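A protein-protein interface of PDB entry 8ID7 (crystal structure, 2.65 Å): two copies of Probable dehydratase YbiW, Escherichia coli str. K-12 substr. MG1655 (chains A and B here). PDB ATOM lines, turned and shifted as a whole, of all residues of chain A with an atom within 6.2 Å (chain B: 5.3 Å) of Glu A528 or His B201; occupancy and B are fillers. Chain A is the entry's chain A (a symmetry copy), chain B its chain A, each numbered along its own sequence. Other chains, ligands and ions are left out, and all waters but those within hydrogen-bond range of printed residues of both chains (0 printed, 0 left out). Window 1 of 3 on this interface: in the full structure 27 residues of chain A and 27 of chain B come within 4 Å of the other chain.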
ATOM      1  N   ILE A  48      17.451  -9.047  -8.387  1.00  0.00           N
ATOM      2  CA  ILE A  48      18.160  -7.816  -8.723  1.00  0.00           C
ATOM      3  C   ILE A  48      17.820  -6.690  -7.776  1.00  0.00           C
ATOM      4  O   ILE A  48      18.740  -5.990  -7.330  1.00  0.00           O
ATOM      5  CB  ILE A  48      17.923  -7.483 -10.218  1.00  0.00           C
ATOM      6  CG1 ILE A  48      18.649  -8.544 -11.068  1.00  0.00           C
ATOM      7  CG2 ILE A  48      18.429  -6.085 -10.510  1.00  0.00           C
ATOM      8  CD1 ILE A  48      17.931  -8.988 -12.386  1.00  0.00           C
ATOM      9  N   MET A 139      17.708  -7.870 -27.972  1.00  0.00           N
ATOM     10  CA  MET A 139      16.291  -7.938 -28.325  1.00  0.00           C
ATOM     11  C   MET A 139      15.961  -7.289 -29.661  1.00  0.00           C
ATOM     12  O   MET A 139      15.257  -7.890 -30.475  1.00  0.00           O
ATOM     13  CB  MET A 139      15.443  -7.277 -27.238  1.00  0.00           C
ATOM     14  CG  MET A 139      15.069  -8.205 -26.111  1.00  0.00           C
ATOM     15  SD  MET A 139      13.664  -7.532 -25.224  1.00  0.00           S
ATOM     16  CE  MET A 139      12.446  -7.604 -26.531  1.00  0.00           C
ATOM     17  N   ASP A 523      12.901   0.572 -22.327  1.00  0.00           N
ATOM     18  CA  ASP A 523      12.207   0.612 -21.044  1.00  0.00           C
ATOM     19  C   ASP A 523      12.072  -0.790 -20.437  1.00  0.00           C
ATOM     20  O   ASP A 523      12.042  -0.938 -19.208  1.00  0.00           O
ATOM     21  CB  ASP A 523      10.826   1.274 -21.198  1.00  0.00           C
ATOM     22  CG  ASP A 523      10.876   2.804 -21.105  1.00  0.00           C
ATOM     23  OD1 ASP A 523      11.987   3.355 -21.006  1.00  0.00           O
ATOM     24  OD2 ASP A 523       9.817   3.478 -21.159  1.00  0.00           O
ATOM     25  N   THR A 524      11.992  -1.839 -21.257  1.00  0.00           N
ATOM     26  CA  THR A 524      11.784  -3.139 -20.625  1.00  0.00           C
ATOM     27  C   THR A 524      13.092  -3.680 -20.076  1.00  0.00           C
ATOM     28  O   THR A 524      13.125  -4.240 -18.979  1.00  0.00           O
ATOM     29  CB  THR A 524      11.134  -4.130 -21.589  1.00  0.00           C
ATOM     30  OG1 THR A 524       9.729  -3.855 -21.680  1.00  0.00           O
ATOM     31  CG2 THR A 524      11.305  -5.532 -21.059  1.00  0.00           C
ATOM     32  N   MET A 525      14.180  -3.460 -20.802  1.00  0.00           N
ATOM     33  CA  MET A 525      15.506  -3.774 -20.289  1.00  0.00           C
ATOM     34  C   MET A 525      15.856  -2.944 -19.045  1.00  0.00           C
ATOM     35  O   MET A 525      16.430  -3.461 -18.079  1.00  0.00           O
ATOM     36  CB  MET A 525      16.503  -3.555 -21.420  1.00  0.00           C
ATOM     37  CG  MET A 525      16.213  -4.468 -22.610  1.00  0.00           C
ATOM     38  SD  MET A 525      16.344  -6.183 -22.102  1.00  0.00           S
ATOM     39  CE  MET A 525      14.626  -6.723 -21.966  1.00  0.00           C
ATOM     40  N   LEU A 526      15.511  -1.659 -19.041  1.00  0.00           N
ATOM     41  CA  LEU A 526      15.773  -0.833 -17.861  1.00  0.00           C
ATOM     42  C   LEU A 526      15.018  -1.329 -16.636  1.00  0.00           C
ATOM     43  O   LEU A 526      15.446  -1.093 -15.499  1.00  0.00           O
ATOM     44  CB  LEU A 526      15.386   0.615 -18.139  1.00  0.00           C
ATOM     45  CG  LEU A 526      16.421   1.451 -18.880  1.00  0.00           C
ATOM     46  CD1 LEU A 526      15.762   2.711 -19.427  1.00  0.00           C
ATOM     47  CD2 LEU A 526      17.538   1.767 -17.934  1.00  0.00           C
ATOM     48  N   GLU A 527      13.884  -1.985 -16.841  1.00  0.00           N
ATOM     49  CA  GLU A 527      13.032  -2.373 -15.738  1.00  0.00           C
ATOM     50  C   GLU A 527      13.343  -3.777 -15.224  1.00  0.00           C
ATOM     51  O   GLU A 527      13.020  -4.099 -14.077  1.00  0.00           O
ATOM     52  CB  GLU A 527      11.577  -2.261 -16.186  1.00  0.00           C
ATOM     53  CG  GLU A 527      10.588  -2.899 -15.272  1.00  0.00           C
ATOM     54  CD  GLU A 527       9.328  -3.216 -15.982  1.00  0.00           C
ATOM     55  OE1 GLU A 527       9.316  -3.123 -17.224  1.00  0.00           O
ATOM     56  OE2 GLU A 527       8.339  -3.553 -15.311  1.00  0.00           O
ATOM     57  N   GLU A 528      13.989  -4.604 -16.029  1.00  0.00           N
ATOM     58  CA  GLU A 528      14.414  -5.915 -15.575  1.00  0.00           C
ATOM     59  C   GLU A 528      15.788  -5.905 -14.931  1.00  0.00           C
ATOM     60  O   GLU A 528      16.090  -6.805 -14.139  1.00  0.00           O
ATOM     61  CB  GLU A 528      14.411  -6.892 -16.748  1.00  0.00           C
ATOM     62  CG  GLU A 528      13.032  -7.083 -17.331  1.00  0.00           C
ATOM     63  CD  GLU A 528      12.968  -8.124 -18.427  1.00  0.00           C
ATOM     64  OE1 GLU A 528      14.042  -8.476 -18.982  1.00  0.00           O
ATOM     65  OE2 GLU A 528      11.831  -8.573 -18.730  1.00  0.00           O
ATOM     66  N   ASN A 529      16.632  -4.914 -15.228  1.00  0.00           N
ATOM     67  CA  ASN A 529      18.019  -4.999 -14.807  1.00  0.00           C
ATOM     68  C   ASN A 529      18.477  -3.933 -13.823  1.00  0.00           C
ATOM     69  O   ASN A 529      19.498  -4.152 -13.168  1.00  0.00           O
ATOM     70  CB  ASN A 529      18.939  -4.972 -16.030  1.00  0.00           C
ATOM     71  CG  ASN A 529      18.724  -6.159 -16.953  1.00  0.00           C
ATOM     72  OD1 ASN A 529      19.327  -7.226 -16.769  1.00  0.00           O
ATOM     73  ND2 ASN A 529      17.872  -5.980 -17.967  1.00  0.00           N
ATOM     74  N   VAL A 530      17.773  -2.808 -13.679  1.00  0.00           N
ATOM     75  CA  VAL A 530      18.338  -1.682 -12.924  1.00  0.00           C
ATOM     76  C   VAL A 530      17.279  -0.942 -12.109  1.00  0.00           C
ATOM     77  O   VAL A 530      17.023   0.250 -12.322  1.00  0.00           O
ATOM     78  CB  VAL A 530      19.085  -0.704 -13.858  1.00  0.00           C
ATOM     79  CG1 VAL A 530      20.181  -1.435 -14.594  1.00  0.00           C
ATOM     80  CG2 VAL A 530      18.136  -0.066 -14.842  1.00  0.00           C
ATOM     81  N   HIS A 531      16.690  -1.634 -11.142  1.00  0.00           N
ATOM     82  CA  HIS A 531      15.727  -1.005 -10.256  1.00  0.00           C
ATOM     83  C   HIS A 531      16.388   0.124  -9.475  1.00  0.00           C
ATOM     84  O   HIS A 531      17.436  -0.058  -8.850  1.00  0.00           O
ATOM     85  CB  HIS A 531      15.146  -2.032  -9.283  1.00  0.00           C
ATOM     86  CG  HIS A 531      14.660  -3.295  -9.922  1.00  0.00           C
ATOM     87  ND1 HIS A 531      15.444  -4.056 -10.756  1.00  0.00           N
ATOM     88  CD2 HIS A 531      13.487  -3.965  -9.795  1.00  0.00           C
ATOM     89  CE1 HIS A 531      14.766  -5.123 -11.145  1.00  0.00           C
ATOM     90  NE2 HIS A 531      13.576  -5.094 -10.571  1.00  0.00           N
ATOM     91  N   LEU B 197       3.011  -4.375 -24.364  1.00  0.00           N
ATOM     92  CA  LEU B 197       3.990  -4.993 -23.483  1.00  0.00           C
ATOM     93  C   LEU B 197       3.939  -6.508 -23.609  1.00  0.00           C
ATOM     94  O   LEU B 197       4.933  -7.147 -23.959  1.00  0.00           O
ATOM     95  CB  LEU B 197       3.745  -4.555 -22.044  1.00  0.00           C
ATOM     96  CG  LEU B 197       4.793  -4.954 -20.997  1.00  0.00           C
ATOM     97  CD1 LEU B 197       6.203  -4.517 -21.383  1.00  0.00           C
ATOM     98  CD2 LEU B 197       4.412  -4.362 -19.644  1.00  0.00           C
ATOM     99  N   GLU B 198       2.756  -7.093 -23.370  1.00  0.00           N
ATOM    100  CA  GLU B 198       2.634  -8.548 -23.329  1.00  0.00           C
ATOM    101  C   GLU B 198       3.070  -9.196 -24.641  1.00  0.00           C
ATOM    102  O   GLU B 198       3.597 -10.320 -24.634  1.00  0.00           O
ATOM    103  CB  GLU B 198       1.197  -8.938 -22.999  1.00  0.00           C
ATOM    104  CG  GLU B 198       0.847  -8.769 -21.530  1.00  0.00           C
ATOM    105  CD  GLU B 198      -0.475  -9.430 -21.158  1.00  0.00           C
ATOM    106  OE1 GLU B 198      -1.352  -9.559 -22.046  1.00  0.00           O
ATOM    107  OE2 GLU B 198      -0.632  -9.830 -19.978  1.00  0.00           O
ATOM    108  N   ASP B 199       2.859  -8.503 -25.776  1.00  0.00           N
ATOM    109  CA  ASP B 199       3.301  -9.028 -27.067  1.00  0.00           C
ATOM    110  C   ASP B 199       4.818  -8.969 -27.202  1.00  0.00           C
ATOM    111  O   ASP B 199       5.414  -9.825 -27.868  1.00  0.00           O
ATOM    112  CB  ASP B 199       2.622  -8.268 -28.217  1.00  0.00           C
ATOM    113  CG  ASP B 199       1.140  -8.661 -28.402  1.00  0.00           C
ATOM    114  OD1 ASP B 199       0.565  -9.297 -27.489  1.00  0.00           O
ATOM    115  OD2 ASP B 199       0.543  -8.351 -29.459  1.00  0.00           O
ATOM    116  N   LEU B 200       5.462  -8.002 -26.552  1.00  0.00           N
ATOM    117  CA  LEU B 200       6.911  -7.898 -26.661  1.00  0.00           C
ATOM    118  C   LEU B 200       7.597  -9.109 -26.052  1.00  0.00           C
ATOM    119  O   LEU B 200       8.578  -9.615 -26.609  1.00  0.00           O
ATOM    120  CB  LEU B 200       7.414  -6.621 -25.992  1.00  0.00           C
ATOM    121  CG  LEU B 200       8.927  -6.568 -26.088  1.00  0.00           C
ATOM    122  CD1 LEU B 200       9.289  -6.332 -27.540  1.00  0.00           C
ATOM    123  CD2 LEU B 200       9.553  -5.515 -25.195  1.00  0.00           C
ATOM    124  N   HIS B 201       7.113  -9.567 -24.891  1.00  0.00           N
ATOM    125  CA  HIS B 201       7.616 -10.796 -24.270  1.00  0.00           C
ATOM    126  C   HIS B 201       7.129 -12.036 -25.001  1.00  0.00           C
ATOM    127  O   HIS B 201       7.823 -13.056 -25.031  1.00  0.00           O
ATOM    128  CB  HIS B 201       7.141 -10.899 -22.831  1.00  0.00           C
ATOM    129  CG  HIS B 201       7.794  -9.944 -21.901  1.00  0.00           C
ATOM    130  ND1 HIS B 201       7.081  -8.987 -21.216  1.00  0.00           N
ATOM    131  CD2 HIS B 201       9.080  -9.822 -21.506  1.00  0.00           C
ATOM    132  CE1 HIS B 201       7.908  -8.295 -20.455  1.00  0.00           C
ATOM    133  NE2 HIS B 201       9.128  -8.777 -20.615  1.00  0.00           N
ATOM    134  N   GLY B 202       5.897 -11.996 -25.510  1.00  0.00           N
ATOM    135  CA  GLY B 202       5.368 -13.131 -26.238  1.00  0.00           C
ATOM    136  C   GLY B 202       6.205 -13.512 -27.442  1.00  0.00           C
ATOM    137  O   GLY B 202       6.284 -14.696 -27.794  1.00  0.00           O
ATOM    138  N   GLU B 203       6.834 -12.525 -28.097  1.00  0.00           N
ATOM    139  CA  GLU B 203       7.563 -12.819 -29.323  1.00  0.00           C
ATOM    140  C   GLU B 203       8.942 -13.373 -29.030  1.00  0.00           C
ATOM    141  O   GLU B 203       9.482 -14.125 -29.852  1.00  0.00           O
ATOM    142  CB  GLU B 203       7.668 -11.573 -30.218  1.00  0.00           C
ATOM    143  CG  GLU B 203       8.664 -11.684 -31.417  1.00  0.00           C
ATOM    144  CD  GLU B 203       8.238 -12.653 -32.538  1.00  0.00           C
ATOM    145  OE1 GLU B 203       7.246 -13.404 -32.362  1.00  0.00           O
ATOM    146  OE2 GLU B 203       8.921 -12.678 -33.595  1.00  0.00           O
ATOM    147  N   GLN B 204       9.539 -13.036 -27.883  1.00  0.00           N
ATOM    148  CA  GLN B 204      10.796 -13.697 -27.541  1.00  0.00           C
ATOM    149  C   GLN B 204      10.560 -15.189 -27.380  1.00  0.00           C
ATOM    150  O   GLN B 204      11.265 -16.014 -27.963  1.00  0.00           O
ATOM    151  CB  GLN B 204      11.427 -13.111 -26.271  1.00  0.00           C
ATOM    152  CG  GLN B 204      12.056 -11.719 -26.400  1.00  0.00           C
ATOM    153  CD  GLN B 204      12.757 -11.482 -27.733  1.00  0.00           C
ATOM    154  OE1 GLN B 204      12.107 -11.411 -28.773  1.00  0.00           O
ATOM    155  NE2 GLN B 204      14.083 -11.345 -27.703  1.00  0.00           N
ATOM    156  N   PHE B 205       9.528 -15.557 -26.637  1.00  0.00           N
ATOM    157  CA  PHE B 205       9.240 -16.971 -26.496  1.00  0.00           C
ATOM    158  C   PHE B 205       8.870 -17.613 -27.830  1.00  0.00           C
ATOM    159  O   PHE B 205       9.159 -18.793 -28.041  1.00  0.00           O
ATOM    160  CB  PHE B 205       8.134 -17.195 -25.473  1.00  0.00           C
ATOM    161  CG  PHE B 205       8.034 -18.596 -25.042  1.00  0.00           C
ATOM    162  CD1 PHE B 205       8.948 -19.111 -24.141  1.00  0.00           C
ATOM    163  CD2 PHE B 205       7.070 -19.422 -25.566  1.00  0.00           C
ATOM    164  CE1 PHE B 205       8.895 -20.420 -23.741  1.00  0.00           C
ATOM    165  CE2 PHE B 205       7.003 -20.735 -25.179  1.00  0.00           C
ATOM    166  CZ  PHE B 205       7.931 -21.234 -24.260  1.00  0.00           C
ATOM    167  N   ALA B 546       1.747 -17.822 -26.113  1.00  0.00           N
ATOM    168  CA  ALA B 546       3.143 -17.430 -26.254  1.00  0.00           C
ATOM    169  C   ALA B 546       3.852 -17.344 -24.903  1.00  0.00           C
ATOM    170  O   ALA B 546       4.487 -16.347 -24.573  1.00  0.00           O
ATOM    171  CB  ALA B 546       3.250 -16.123 -27.024  1.00  0.00           C
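NE2 of His B201 sits at hydrogen-bond distance from OE2 of Glu A528, at 3.3 Å.
Met A139 touches Leu B200 (CE to CD1, 3.6 Å). Met A139 touches Gln B204. CD1 of Leu B197 touches OG1 of Thr A524, at 3.6 Å. Thr A524 touches Leu B200 (OG1 to CD2, 3.9 Å). CG2 of Thr A524 touches NE2 of His B201 (3.9 Å).
Printed residues of chain B within 4 Å of Met A139: Leu B200 (3.6 Å) and Gln B204 (3.7 Å). Leu A526 touches none of the printed residues of chain B. Of the printed residues of chain B, Glu A528 touches His B201. Of the printed residues of chain A, Leu B197 touches Thr A524. His B201 touches just these residues of chain A: Thr A524 (3.9 Å) and Glu A528 (3.3 Å). Phe B205 touches none of the printed residues of chain A. The nearest printed residue of chain B that does not touch Thr A524 is Glu B198 (7.9 Å).
Of the 11 printed residues of chain A, 3 touch a printed residue of chain B. Hydrophobic or aromatic side chains of chain B that line the printed part of chain A: Leu B197, Leu B200 and His B201.
No position is printed for both chains.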
